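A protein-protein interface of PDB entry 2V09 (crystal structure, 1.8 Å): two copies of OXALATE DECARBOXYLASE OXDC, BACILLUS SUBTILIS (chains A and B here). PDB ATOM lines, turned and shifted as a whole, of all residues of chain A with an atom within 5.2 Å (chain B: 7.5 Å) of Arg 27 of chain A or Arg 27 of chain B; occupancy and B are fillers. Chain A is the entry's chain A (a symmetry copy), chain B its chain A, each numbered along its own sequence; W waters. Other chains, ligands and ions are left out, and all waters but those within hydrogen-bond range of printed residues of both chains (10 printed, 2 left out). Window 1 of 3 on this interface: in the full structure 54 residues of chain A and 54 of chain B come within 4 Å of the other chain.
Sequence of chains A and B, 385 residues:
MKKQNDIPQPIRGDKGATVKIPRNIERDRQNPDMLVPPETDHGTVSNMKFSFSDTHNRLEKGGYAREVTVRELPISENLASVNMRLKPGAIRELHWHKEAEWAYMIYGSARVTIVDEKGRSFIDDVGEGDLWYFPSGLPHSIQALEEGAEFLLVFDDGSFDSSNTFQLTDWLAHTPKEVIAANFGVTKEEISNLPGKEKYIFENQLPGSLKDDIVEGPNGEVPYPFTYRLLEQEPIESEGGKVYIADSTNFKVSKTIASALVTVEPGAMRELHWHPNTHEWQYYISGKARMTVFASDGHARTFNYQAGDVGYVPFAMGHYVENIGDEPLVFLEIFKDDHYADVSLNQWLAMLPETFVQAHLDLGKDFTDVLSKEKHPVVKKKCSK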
ATOM      1  N   ASN A  24       7.030  -3.216 -12.032  1.00  0.00           N
ATOM      2  CA  ASN A  24       6.924  -4.576 -12.532  1.00  0.00           C
ATOM      3  C   ASN A  24       7.400  -5.587 -11.523  1.00  0.00           C
ATOM      4  O   ASN A  24       8.571  -5.973 -11.483  1.00  0.00           O
ATOM      5  CB  ASN A  24       7.691  -4.713 -13.852  1.00  0.00           C
ATOM      6  CG  ASN A  24       7.251  -5.924 -14.656  1.00  0.00           C
ATOM      7  OD1 ASN A  24       6.931  -6.986 -14.096  1.00  0.00           O
ATOM      8  ND2 ASN A  24       7.199  -5.761 -16.001  1.00  0.00           N
ATOM      9  N   ILE A  25       6.477  -6.012 -10.659  1.00  0.00           N
ATOM     10  CA  ILE A  25       6.855  -6.841  -9.538  1.00  0.00           C
ATOM     11  C   ILE A  25       7.292  -8.228 -10.007  1.00  0.00           C
ATOM     12  O   ILE A  25       8.207  -8.793  -9.419  1.00  0.00           O
ATOM     13  CB  ILE A  25       5.740  -6.900  -8.475  1.00  0.00           C
ATOM     14  CG1 ILE A  25       6.326  -7.387  -7.168  1.00  0.00           C
ATOM     15  CG2 ILE A  25       4.649  -7.791  -8.909  1.00  0.00           C
ATOM     16  CD1 ILE A  25       7.238  -6.357  -6.533  1.00  0.00           C
ATOM     17  N   GLU A  26       6.684  -8.780 -11.067  1.00  0.00           N
ATOM     18  CA  GLU A  26       7.107 -10.109 -11.597  1.00  0.00           C
ATOM     19  C   GLU A  26       8.527 -10.120 -12.106  1.00  0.00           C
ATOM     20  O   GLU A  26       9.293 -11.042 -11.833  1.00  0.00           O
ATOM     21  CB  GLU A  26       6.205 -10.630 -12.724  1.00  0.00           C
ATOM     22  CG  GLU A  26       4.780 -10.889 -12.289  1.00  0.00           C
ATOM     23  CD  GLU A  26       3.904  -9.627 -12.167  1.00  0.00           C
ATOM     24  OE1 GLU A  26       4.296  -8.426 -12.498  1.00  0.00           O
ATOM     25  OE2 GLU A  26       2.781  -9.862 -11.675  1.00  0.00           O
ATOM     26  N   ARG A  27       8.904  -9.073 -12.837  1.00  0.00           N
ATOM     27  CA  ARG A  27      10.290  -8.911 -13.254  1.00  0.00           C
ATOM     28  C   ARG A  27      11.253  -8.683 -12.095  1.00  0.00           C
ATOM     29  O   ARG A  27      12.325  -9.279 -12.053  1.00  0.00           O
ATOM     30  CB  ARG A  27      10.457  -7.826 -14.324  1.00  0.00           C
ATOM     31  CG  ARG A  27      10.057  -8.277 -15.674  1.00  0.00           C
ATOM     32  CD  ARG A  27      10.294  -7.262 -16.774  1.00  0.00           C
ATOM     33  NE  ARG A  27       9.396  -7.665 -17.870  1.00  0.00           N
ATOM     34  CZ  ARG A  27       9.711  -7.829 -19.150  1.00  0.00           C
ATOM     35  NH1 ARG A  27      10.895  -7.508 -19.602  1.00  0.00           N
ATOM     36  NH2 ARG A  27       8.767  -8.208 -19.993  1.00  0.00           N
ATOM     37  N   ASP A  28      10.873  -7.858 -11.124  1.00  0.00           N
ATOM     38  CA  ASP A  28      11.669  -7.688  -9.923  1.00  0.00           C
ATOM     39  C   ASP A  28      11.950  -8.999  -9.187  1.00  0.00           C
ATOM     40  O   ASP A  28      13.062  -9.203  -8.764  1.00  0.00           O
ATOM     41  CB  ASP A  28      11.055  -6.656  -8.958  1.00  0.00           C
ATOM     42  CG  ASP A  28      11.075  -5.227  -9.510  1.00  0.00           C
ATOM     43  OD1 ASP A  28      11.815  -4.935 -10.470  1.00  0.00           O
ATOM     44  OD2 ASP A  28      10.301  -4.377  -8.979  1.00  0.00           O
ATOM     45  N   ARG A  29      10.953  -9.874  -9.072  1.00  0.00           N
ATOM     46  CA  ARG A  29      11.129 -11.190  -8.473  1.00  0.00           C
ATOM     47  C   ARG A  29      12.096 -12.085  -9.246  1.00  0.00           C
ATOM     48  O   ARG A  29      12.759 -12.922  -8.632  1.00  0.00           O
ATOM     49  CB  ARG A  29       9.780 -11.881  -8.338  1.00  0.00           C
ATOM     50  CG  ARG A  29       8.919 -11.294  -7.239  1.00  0.00           C
ATOM     51  CD  ARG A  29       7.585 -12.058  -7.204  1.00  0.00           C
ATOM     52  NE  ARG A  29       6.593 -11.413  -6.332  1.00  0.00           N
ATOM     53  CZ  ARG A  29       5.301 -11.240  -6.633  1.00  0.00           C
ATOM     54  NH1 ARG A  29       4.763 -11.595  -7.825  1.00  0.00           N
ATOM     55  NH2 ARG A  29       4.519 -10.629  -5.732  1.00  0.00           N
ATOM     56  N   GLN A  30      12.149 -11.928 -10.570  1.00  0.00           N
ATOM     57  CA  GLN A  30      13.033 -12.688 -11.408  1.00  0.00           C
ATOM     58  C   GLN A  30      14.472 -12.167 -11.300  1.00  0.00           C
ATOM     59  O   GLN A  30      15.418 -12.926 -11.581  1.00  0.00           O
ATOM     60  CB  GLN A  30      12.575 -12.662 -12.878  1.00  0.00           C
ATOM     61  CG  GLN A  30      11.233 -13.328 -13.085  1.00  0.00           C
ATOM     62  CD  GLN A  30      10.902 -13.644 -14.514  1.00  0.00           C
ATOM     63  OE1 GLN A  30      11.543 -13.167 -15.431  1.00  0.00           O
ATOM     64  NE2 GLN A  30       9.873 -14.464 -14.704  1.00  0.00           N
ATOM     65  N   ASN A  31      14.617 -10.893 -10.919  1.00  0.00           N
ATOM     66  CA  ASN A  31      15.927 -10.238 -10.923  1.00  0.00           C
ATOM     67  C   ASN A  31      16.379  -9.790  -9.516  1.00  0.00           C
ATOM     68  O   ASN A  31      16.700  -8.599  -9.341  1.00  0.00           O
ATOM     69  CB  ASN A  31      15.891  -9.030 -11.862  1.00  0.00           C
ATOM     70  CG  ASN A  31      15.616  -9.414 -13.312  1.00  0.00           C
ATOM     71  OD1 ASN A  31      15.949 -10.530 -13.777  1.00  0.00           O
ATOM     72  ND2 ASN A  31      15.029  -8.495 -14.029  1.00  0.00           N
ATOM     73  N   LYS A  49      22.173  -9.243 -20.618  1.00  0.00           N
ATOM     74  CA  LYS A  49      21.007 -10.151 -20.414  1.00  0.00           C
ATOM     75  C   LYS A  49      19.852  -9.800 -21.321  1.00  0.00           C
ATOM     76  O   LYS A  49      19.489  -8.641 -21.412  1.00  0.00           O
ATOM     77  CB  LYS A  49      20.577 -10.041 -18.937  1.00  0.00           C
ATOM     78  CG  LYS A  49      19.242 -10.620 -18.549  1.00  0.00           C
ATOM     79  CD  LYS A  49      18.955 -10.106 -17.099  1.00  0.00           C
ATOM     80  CE  LYS A  49      17.475 -10.239 -16.725  1.00  0.00           C
ATOM     81  NZ  LYS A  49      17.158 -11.614 -16.315  1.00  0.00           N
ATOM     82  N   SER A  51      15.913 -11.722 -22.698  1.00  0.00           N
ATOM     83  CA  SER A  51      15.046 -12.871 -22.763  1.00  0.00           C
ATOM     84  C   SER A  51      14.413 -13.040 -24.146  1.00  0.00           C
ATOM     85  O   SER A  51      13.879 -12.116 -24.682  1.00  0.00           O
ATOM     86  CB  SER A  51      13.951 -12.738 -21.742  1.00  0.00           C
ATOM     87  OG  SER A  51      13.101 -13.874 -21.814  1.00  0.00           O
ATOM     88  N   SER A  53      11.614 -14.389 -24.454  1.00  0.00           N
ATOM     89  CA  SER A  53      10.243 -14.000 -24.157  1.00  0.00           C
ATOM     90  C   SER A  53       9.939 -12.528 -24.401  1.00  0.00           C
ATOM     91  O   SER A  53       8.769 -12.153 -24.538  1.00  0.00           O
ATOM     92  CB  SER A  53       9.905 -14.336 -22.702  1.00  0.00           C
ATOM     93  OG  SER A  53       9.695 -15.709 -22.592  1.00  0.00           O
ATOM     94  N   ASP A  54      10.979 -11.694 -24.491  1.00  0.00           N
ATOM     95  CA  ASP A  54      10.801 -10.288 -24.851  1.00  0.00           C
ATOM     96  C   ASP A  54      11.022  -9.976 -26.355  1.00  0.00           C
ATOM     97  O   ASP A  54      11.352  -8.842 -26.742  1.00  0.00           O
ATOM     98  CB  ASP A  54      11.737  -9.449 -23.982  1.00  0.00           C
ATOM     99  CG  ASP A  54      11.293  -9.378 -22.510  1.00  0.00           C
ATOM    100  OD1 ASP A  54      10.104  -9.165 -22.248  1.00  0.00           O
ATOM    101  OD2 ASP A  54      12.158  -9.497 -21.625  1.00  0.00           O
ATOM    102  N   PRO B   8      -0.191 -19.520 -21.726  1.00  0.00           N
ATOM    103  CA  PRO B   8      -0.297 -19.068 -23.128  1.00  0.00           C
ATOM    104  C   PRO B   8       0.642 -19.854 -24.078  1.00  0.00           C
ATOM    105  O   PRO B   8       1.738 -20.325 -23.689  1.00  0.00           O
ATOM    106  CB  PRO B   8       0.109 -17.597 -23.051  1.00  0.00           C
ATOM    107  CG  PRO B   8       0.958 -17.470 -21.816  1.00  0.00           C
ATOM    108  CD  PRO B   8       0.432 -18.500 -20.854  1.00  0.00           C
ATOM    109  N   ARG B  23      10.857 -22.357 -20.323  1.00  0.00           N
ATOM    110  CA  ARG B  23      10.422 -21.051 -20.799  1.00  0.00           C
ATOM    111  C   ARG B  23      10.095 -20.140 -19.631  1.00  0.00           C
ATOM    112  O   ARG B  23       9.995 -20.587 -18.477  1.00  0.00           O
ATOM    113  CB  ARG B  23       9.176 -21.161 -21.718  1.00  0.00           C
ATOM    114  CG  ARG B  23       7.949 -21.667 -20.977  1.00  0.00           C
ATOM    115  CD  ARG B  23       6.766 -22.076 -21.883  1.00  0.00           C
ATOM    116  NE  ARG B  23       6.175 -20.920 -22.467  1.00  0.00           N
ATOM    117  CZ  ARG B  23       4.922 -20.863 -22.928  1.00  0.00           C
ATOM    118  NH1 ARG B  23       4.129 -21.913 -22.864  1.00  0.00           N
ATOM    119  NH2 ARG B  23       4.486 -19.743 -23.429  1.00  0.00           N
ATOM    120  N   ASN B  24       9.882 -18.871 -19.976  1.00  0.00           N
ATOM    121  CA  ASN B  24       9.522 -17.814 -19.046  1.00  0.00           C
ATOM    122  C   ASN B  24       8.068 -17.437 -19.156  1.00  0.00           C
ATOM    123  O   ASN B  24       7.675 -16.546 -19.912  1.00  0.00           O
ATOM    124  CB  ASN B  24      10.423 -16.593 -19.263  1.00  0.00           C
ATOM    125  CG  ASN B  24      10.435 -15.661 -18.065  1.00  0.00           C
ATOM    126  OD1 ASN B  24       9.411 -15.471 -17.387  1.00  0.00           O
ATOM    127  ND2 ASN B  24      11.626 -15.085 -17.768  1.00  0.00           N
ATOM    128  N   ILE B  25       7.233 -18.154 -18.402  1.00  0.00           N
ATOM    129  CA  ILE B  25       5.805 -18.008 -18.554  1.00  0.00           C
ATOM    130  C   ILE B  25       5.339 -16.639 -18.060  1.00  0.00           C
ATOM    131  O   ILE B  25       4.431 -16.070 -18.653  1.00  0.00           O
ATOM    132  CB  ILE B  25       5.040 -19.169 -17.888  1.00  0.00           C
ATOM    133  CG1 ILE B  25       3.632 -19.216 -18.437  1.00  0.00           C
ATOM    134  CG2 ILE B  25       5.012 -19.004 -16.423  1.00  0.00           C
ATOM    135  CD1 ILE B  25       3.597 -19.676 -19.880  1.00  0.00           C
ATOM    136  N   GLU B  26       5.956 -16.082 -17.007  1.00  0.00           N
ATOM    137  CA  GLU B  26       5.575 -14.725 -16.516  1.00  0.00           C
ATOM    138  C   GLU B  26       5.813 -13.637 -17.534  1.00  0.00           C
ATOM    139  O   GLU B  26       4.973 -12.763 -17.738  1.00  0.00           O
ATOM    140  CB  GLU B  26       6.298 -14.319 -15.225  1.00  0.00           C
ATOM    141  CG  GLU B  26       5.966 -15.202 -14.042  1.00  0.00           C
ATOM    142  CD  GLU B  26       6.694 -16.561 -14.027  1.00  0.00           C
ATOM    143  OE1 GLU B  26       7.602 -16.916 -14.894  1.00  0.00           O
ATOM    144  OE2 GLU B  26       6.293 -17.314 -13.117  1.00  0.00           O
ATOM    145  N   ARG B  27       6.961 -13.694 -18.207  1.00  0.00           N
ATOM    146  CA  ARG B  27       7.227 -12.783 -19.311  1.00  0.00           C
ATOM    147  C   ARG B  27       6.302 -12.986 -20.506  1.00  0.00           C
ATOM    148  O   ARG B  27       5.800 -12.020 -21.072  1.00  0.00           O
ATOM    149  CB  ARG B  27       8.697 -12.806 -19.748  1.00  0.00           C
ATOM    150  CG  ARG B  27       9.582 -12.040 -18.844  1.00  0.00           C
ATOM    151  CD  ARG B  27      11.027 -11.963 -19.293  1.00  0.00           C
ATOM    152  NE  ARG B  27      11.792 -11.646 -18.075  1.00  0.00           N
ATOM    153  CZ  ARG B  27      12.699 -10.688 -17.921  1.00  0.00           C
ATOM    154  NH1 ARG B  27      13.110  -9.974 -18.937  1.00  0.00           N
ATOM    155  NH2 ARG B  27      13.279 -10.545 -16.741  1.00  0.00           N
ATOM    156  N   ASP B  28       6.032 -14.234 -20.878  1.00  0.00           N
ATOM    157  CA  ASP B  28       5.060 -14.517 -21.917  1.00  0.00           C
ATOM    158  C   ASP B  28       3.680 -13.921 -21.640  1.00  0.00           C
ATOM    159  O   ASP B  28       3.088 -13.379 -22.542  1.00  0.00           O
ATOM    160  CB  ASP B  28       4.941 -16.026 -22.207  1.00  0.00           C
ATOM    161  CG  ASP B  28       6.205 -16.622 -22.836  1.00  0.00           C
ATOM    162  OD1 ASP B  28       7.063 -15.876 -23.348  1.00  0.00           O
ATOM    163  OD2 ASP B  28       6.352 -17.879 -22.790  1.00  0.00           O
ATOM    164  N   ARG B  29       3.204 -14.002 -20.400  1.00  0.00           N
ATOM    165  CA  ARG B  29       1.944 -13.390 -20.000  1.00  0.00           C
ATOM    166  C   ARG B  29       1.944 -11.867 -20.118  1.00  0.00           C
ATOM    167  O   ARG B  29       0.889 -11.285 -20.371  1.00  0.00           O
ATOM    168  CB  ARG B  29       1.599 -13.799 -18.576  1.00  0.00           C
ATOM    169  CG  ARG B  29       1.146 -15.240 -18.465  1.00  0.00           C
ATOM    170  CD  ARG B  29       0.839 -15.541 -16.989  1.00  0.00           C
ATOM    171  NE  ARG B  29       0.618 -16.974 -16.743  1.00  0.00           N
ATOM    172  CZ  ARG B  29       1.114 -17.663 -15.711  1.00  0.00           C
ATOM    173  NH1 ARG B  29       1.942 -17.120 -14.785  1.00  0.00           N
ATOM    174  NH2 ARG B  29       0.826 -18.970 -15.626  1.00  0.00           N
ATOM    175  N   GLN B  30       3.103 -11.237 -19.909  1.00  0.00           N
ATOM    176  CA  GLN B  30       3.242  -9.813 -20.014  1.00  0.00           C
ATOM    177  C   GLN B  30       3.282  -9.374 -21.483  1.00  0.00           C
ATOM    178  O   GLN B  30       2.963  -8.207 -21.780  1.00  0.00           O
ATOM    179  CB  GLN B  30       4.504  -9.316 -19.284  1.00  0.00           C
ATOM    180  CG  GLN B  30       4.451  -9.557 -17.792  1.00  0.00           C
ATOM    181  CD  GLN B  30       5.468  -8.795 -16.995  1.00  0.00           C
ATOM    182  OE1 GLN B  30       6.409  -8.244 -17.535  1.00  0.00           O
ATOM    183  NE2 GLN B  30       5.275  -8.769 -15.681  1.00  0.00           N
ATOM    184  N   ASN B  31       3.684 -10.291 -22.369  1.00  0.00           N
ATOM    185  CA  ASN B  31       3.907  -9.952 -23.775  1.00  0.00           C
ATOM    186  C   ASN B  31       2.968 -10.715 -24.734  1.00  0.00           C
ATOM    187  O   ASN B  31       3.470 -11.373 -25.667  1.00  0.00           O
ATOM    188  CB  ASN B  31       5.365 -10.236 -24.145  1.00  0.00           C
ATOM    189  CG  ASN B  31       6.355  -9.388 -23.354  1.00  0.00           C
ATOM    190  OD1 ASN B  31       6.054  -8.251 -22.918  1.00  0.00           O
ATOM    191  ND2 ASN B  31       7.532  -9.924 -23.180  1.00  0.00           N
ATOM    192  N   PRO B  32       1.630 -10.603 -24.530  1.00  0.00           N
ATOM    193  CA  PRO B  32       0.707 -11.475 -25.333  1.00  0.00           C
ATOM    194  C   PRO B  32       0.799 -11.208 -26.854  1.00  0.00           C
ATOM    195  O   PRO B  32       0.694 -12.156 -27.675  1.00  0.00           O
ATOM    196  CB  PRO B  32      -0.681 -11.138 -24.753  1.00  0.00           C
ATOM    197  CG  PRO B  32      -0.541  -9.731 -24.247  1.00  0.00           C
ATOM    198  CD  PRO B  32       0.862  -9.700 -23.657  1.00  0.00           C
ATOM    199  N   MET B  34       3.502 -10.290 -28.470  1.00  0.00           N
ATOM    200  CA  MET B  34       4.821 -10.698 -28.913  1.00  0.00           C
ATOM    201  C   MET B  34       4.883 -12.222 -29.045  1.00  0.00           C
ATOM    202  O   MET B  34       5.364 -12.766 -30.043  1.00  0.00           O
ATOM    203  CB  MET B  34       5.883 -10.120 -27.963  1.00  0.00           C
ATOM    204  CG  MET B  34       5.724  -8.537 -27.880  1.00  0.00           C
ATOM    205  SD  MET B  34       6.888  -7.693 -26.879  1.00  0.00           S
ATOM    206  CE  MET B  34       8.348  -7.980 -27.914  1.00  0.00           C
ATOM    207  N   LEU B  35       4.355 -12.931 -28.047  1.00  0.00           N
ATOM    208  CA  LEU B  35       4.245 -14.404 -28.132  1.00  0.00           C
ATOM    209  C   LEU B  35       3.290 -14.775 -29.311  1.00  0.00           C
ATOM    210  O   LEU B  35       3.541 -15.719 -30.073  1.00  0.00           O
ATOM    211  CB  LEU B  35       3.680 -14.976 -26.828  1.00  0.00           C
ATOM    212  CG  LEU B  35       3.694 -16.504 -26.762  1.00  0.00           C
ATOM    213  CD1 LEU B  35       5.149 -16.997 -26.607  1.00  0.00           C
ATOM    214  CD2 LEU B  35       2.770 -17.048 -25.635  1.00  0.00           C
ATOM    215  N   LYS B  49      11.602  -1.894 -26.916  1.00  0.00           N
ATOM    216  CA  LYS B  49      11.055  -2.098 -25.543  1.00  0.00           C
ATOM    217  C   LYS B  49      12.129  -2.502 -24.562  1.00  0.00           C
ATOM    218  O   LYS B  49      12.910  -3.390 -24.854  1.00  0.00           O
ATOM    219  CB  LYS B  49       9.970  -3.191 -25.626  1.00  0.00           C
ATOM    220  CG  LYS B  49       9.483  -3.796 -24.335  1.00  0.00           C
ATOM    221  CD  LYS B  49       8.635  -5.048 -24.740  1.00  0.00           C
ATOM    222  CE  LYS B  49       8.431  -6.008 -23.564  1.00  0.00           C
ATOM    223  NZ  LYS B  49       7.349  -5.541 -22.686  1.00  0.00           N
ATOM    224  N   PHE B  50      12.166  -1.876 -23.393  1.00  0.00           N
ATOM    225  CA  PHE B  50      13.110  -2.308 -22.344  1.00  0.00           C
ATOM    226  C   PHE B  50      12.508  -1.926 -20.968  1.00  0.00           C
ATOM    227  O   PHE B  50      11.977  -0.780 -20.838  1.00  0.00           O
ATOM    228  CB  PHE B  50      14.517  -1.715 -22.536  1.00  0.00           C
ATOM    229  CG  PHE B  50      15.604  -2.557 -21.921  1.00  0.00           C
ATOM    230  CD1 PHE B  50      15.932  -2.359 -20.585  1.00  0.00           C
ATOM    231  CD2 PHE B  50      16.216  -3.614 -22.626  1.00  0.00           C
ATOM    232  CE1 PHE B  50      16.855  -3.137 -19.952  1.00  0.00           C
ATOM    233  CE2 PHE B  50      17.205  -4.436 -21.959  1.00  0.00           C
ATOM    234  CZ  PHE B  50      17.504  -4.185 -20.640  1.00  0.00           C
ATOM    235  N   SER B  51      12.614  -2.823 -20.004  1.00  0.00           N
ATOM    236  CA  SER B  51      12.112  -2.563 -18.679  1.00  0.00           C
ATOM    237  C   SER B  51      13.213  -2.090 -17.726  1.00  0.00           C
ATOM    238  O   SER B  51      14.240  -2.694 -17.645  1.00  0.00           O
ATOM    239  CB  SER B  51      11.490  -3.811 -18.119  1.00  0.00           C
ATOM    240  OG  SER B  51      10.999  -3.545 -16.812  1.00  0.00           O
ATOM    241  N   PHE B  52      12.898  -1.052 -16.946  1.00  0.00           N
ATOM    242  CA  PHE B  52      13.775  -0.641 -15.789  1.00  0.00           C
ATOM    243  C   PHE B  52      14.012  -1.787 -14.789  1.00  0.00           C
ATOM    244  O   PHE B  52      15.090  -1.890 -14.170  1.00  0.00           O
ATOM    245  CB  PHE B  52      13.253   0.589 -15.051  1.00  0.00           C
ATOM    246  CG  PHE B  52      13.659   1.907 -15.652  1.00  0.00           C
ATOM    247  CD1 PHE B  52      14.927   2.420 -15.466  1.00  0.00           C
ATOM    248  CD2 PHE B  52      12.731   2.657 -16.381  1.00  0.00           C
ATOM    249  CE1 PHE B  52      15.268   3.651 -15.989  1.00  0.00           C
ATOM    250  CE2 PHE B  52      13.073   3.927 -16.908  1.00  0.00           C
ATOM    251  CZ  PHE B  52      14.358   4.401 -16.740  1.00  0.00           C
ATOM    252  N   SER B  53      13.023  -2.681 -14.666  1.00  0.00           N
ATOM    253  CA  SER B  53      13.168  -3.867 -13.834  1.00  0.00           C
ATOM    254  C   SER B  53      14.244  -4.838 -14.302  1.00  0.00           C
ATOM    255  O   SER B  53      14.709  -5.671 -13.516  1.00  0.00           O
ATOM    256  CB  SER B  53      11.835  -4.616 -13.751  1.00  0.00           C
ATOM    257  OG  SER B  53      10.984  -3.931 -12.885  1.00  0.00           O
ATOM    258  N   ASP B  54      14.671  -4.719 -15.562  1.00  0.00           N
ATOM    259  CA  ASP B  54      15.789  -5.515 -16.068  1.00  0.00           C
ATOM    260  C   ASP B  54      17.161  -4.792 -16.031  1.00  0.00           C
ATOM    261  O   ASP B  54      18.085  -5.111 -16.798  1.00  0.00           O
ATOM    262  CB  ASP B  54      15.453  -5.964 -17.489  1.00  0.00           C
ATOM    263  CG  ASP B  54      14.351  -7.038 -17.538  1.00  0.00           C
ATOM    264  OD1 ASP B  54      14.402  -7.991 -16.751  1.00  0.00           O
ATOM    265  OD2 ASP B  54      13.463  -6.935 -18.401  1.00  0.00           O
ATOM    266  N   ASN B 304       4.420  -4.942 -26.527  1.00  0.00           N
ATOM    267  CA  ASN B 304       3.674  -4.717 -25.296  1.00  0.00           C
ATOM    268  C   ASN B 304       4.477  -3.933 -24.302  1.00  0.00           C
ATOM    269  O   ASN B 304       5.694  -4.139 -24.171  1.00  0.00           O
ATOM    270  CB  ASN B 304       3.292  -6.040 -24.640  1.00  0.00           C
ATOM    271  CG  ASN B 304       2.251  -6.798 -25.418  1.00  0.00           C
ATOM    272  OD1 ASN B 304       2.536  -7.870 -25.937  1.00  0.00           O
ATOM    273  ND2 ASN B 304       1.047  -6.230 -25.528  1.00  0.00           N
ATOM    274  N   GLN B 306       4.149  -2.047 -20.165  1.00  0.00           N
ATOM    275  CA  GLN B 306       3.474  -1.774 -18.883  1.00  0.00           C
ATOM    276  C   GLN B 306       4.346  -0.868 -18.011  1.00  0.00           C
ATOM    277  O   GLN B 306       5.460  -0.501 -18.434  1.00  0.00           O
ATOM    278  CB  GLN B 306       3.084  -3.089 -18.227  1.00  0.00           C
ATOM    279  CG  GLN B 306       4.206  -3.991 -17.789  1.00  0.00           C
ATOM    280  CD  GLN B 306       3.614  -5.266 -17.205  1.00  0.00           C
ATOM    281  OE1 GLN B 306       3.052  -6.132 -17.934  1.00  0.00           O
ATOM    282  NE2 GLN B 306       3.655  -5.352 -15.882  1.00  0.00           N
ATOM    283  N   ALA B 307       3.822  -0.499 -16.829  1.00  0.00           N
ATOM    284  CA  ALA B 307       4.546   0.385 -15.903  1.00  0.00           C
ATOM    285  C   ALA B 307       6.011  -0.051 -15.793  1.00  0.00           C
ATOM    286  O   ALA B 307       6.289  -1.236 -15.577  1.00  0.00           O
ATOM    287  CB  ALA B 307       3.887   0.382 -14.517  1.00  0.00           C
ATOM    288  N   ASP B 309       8.333   0.409 -18.214  1.00  0.00           N
ATOM    289  CA  ASP B 309       8.921   0.108 -19.531  1.00  0.00           C
ATOM    290  C   ASP B 309       9.283   1.386 -20.270  1.00  0.00           C
ATOM    291  O   ASP B 309       8.589   2.423 -20.184  1.00  0.00           O
ATOM    292  CB  ASP B 309       7.969  -0.653 -20.422  1.00  0.00           C
ATOM    293  CG  ASP B 309       7.853  -2.129 -20.044  1.00  0.00           C
ATOM    294  OD1 ASP B 309       8.738  -2.636 -19.322  1.00  0.00           O
ATOM    295  OD2 ASP B 309       6.853  -2.744 -20.459  1.00  0.00           O
HETATM  296  O   HOH W   1       9.380  -1.736 -12.510  1.00  0.00           O
HETATM  297  O   HOH W   2       6.769 -13.939 -25.366  1.00  0.00           O
HETATM  298  O   HOH W   3      11.711  -6.299 -25.428  1.00  0.00           O
HETATM  299  O   HOH W   4      10.837 -18.205 -22.542  1.00  0.00           O
HETATM  300  O   HOH W   5       8.173  -2.968 -16.701  1.00  0.00           O
HETATM  301  O   HOH W   6       2.655  -7.156 -14.093  1.00  0.00           O
HETATM  302  O   HOH W   7      14.595  -5.257 -10.742  1.00  0.00           O
HETATM  303  O   HOH W   8       9.819 -17.814 -13.828  1.00  0.00           O
HETATM  304  O   HOH W   9      13.677 -15.913 -19.853  1.00  0.00           O
HETATM  305  O   HOH W  10      18.432  -7.197 -18.762  1.00  0.00           O
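ND2 of Asn 31 of chain B sits at hydrogen-bond distance from O of Arg 27 of chain B. The guanidinium group of Arg 27 of chain A lies within salt-bridge range of the side-chain carboxylate of Asp 54 of chain A, at 2.8 Å.
Of chain B, only Arg 27, Gln 30, Asn 31, Ser 51, Ser 53 and Asp 54 come within 4 Å of Arg 27 of chain A. Arg 27 of chain B touches just these residues of chain A: Arg 27, Gln 30, Asn 31, Ser 51, Ser 53 and Asp 54. Printed residues of chain B within 4 Å of Ser 51 of chain A: Arg 27 (3.8 Å). Printed residues of chain B within 4 Å of Glu 26 of chain A: Gln 30. Ile 25 of chain B touches none of the printed residues of chain A. The nearest residue of chain A that does not touch Arg 27 of chain B is Lys 49 of chain A (4.05 Å).
Arg 27 of chain A touches Asn 31 of chain B, and with the chains exchanged Asn 31 of chain A touches Arg 27 of chain B. Positions printed for both chains: 24, 25, 26, 27, 28, 29, 30, 31, 49, 51, 53 and 54.
The backbone carbonyl oxygen (O) of Asn 24 of chain B is in hydrogen-bond range of the side-chain hydroxyl (OG) of Ser 53 of chain A (3.5 Å). NE2 of Gln 30 of chain A sits at hydrogen-bond distance from OE1 of Glu 26 of chain B (3.3 Å). The guanidinium group (NH1) of Arg 27 of chain B lies within salt-bridge range of the side-chain carboxylate (OD2) of Asp 54 of chain A (2.9 Å). OD1 of Asp 28 of chain B lies within hydrogen-bond range of OG of Ser 53 of chain A (2.7 Å). The side-chain amide nitrogen of Gln 30 of chain B sits at hydrogen-bond distance from the side-chain amide oxygen of Asn 24 of chain A (2.9 Å). O of Ser 53 of chain B lies within hydrogen-bond range of ND2 of Asn 31 of chain A (2.9 Å). OD2 of Asp 54 of chain B is in salt-bridge range of NH1 of Arg 27 of chain A (2.9 Å).
Water W8 bridges the side-chain carboxylate of Glu 26 of chain B and the side-chain amide nitrogen of Gln 30 of chain A. Water W10 lies within hydrogen-bond range of O of Asp 54 of chain B (2.9 Å) and O of Lys 49 of chain A (3.2 Å).
Printed residues of chain B that touch a printed residue of chain A: Asn 24, Glu 26, Arg 27, Asp 28, Gln 30, Asn 31, Met 34, Lys 49, Ser 51, Ser 53, Asp 54 and Gln 306. Hydrophobic or aromatic side chains of chain B that line the printed part of chain A: Met 34. Of the 12 printed residues of chain A, 10 touch a printed residue of chain B. Among the printed residues, Asp or Glu carboxylates within 4 Å of a Lys or Arg side-chain nitrogen of the other chain: Arg 27 of chain A with Asp 54 of chain B (2.9 Å) and Asp 54 of chain A with Arg 27 of chain B (2.9 Å).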
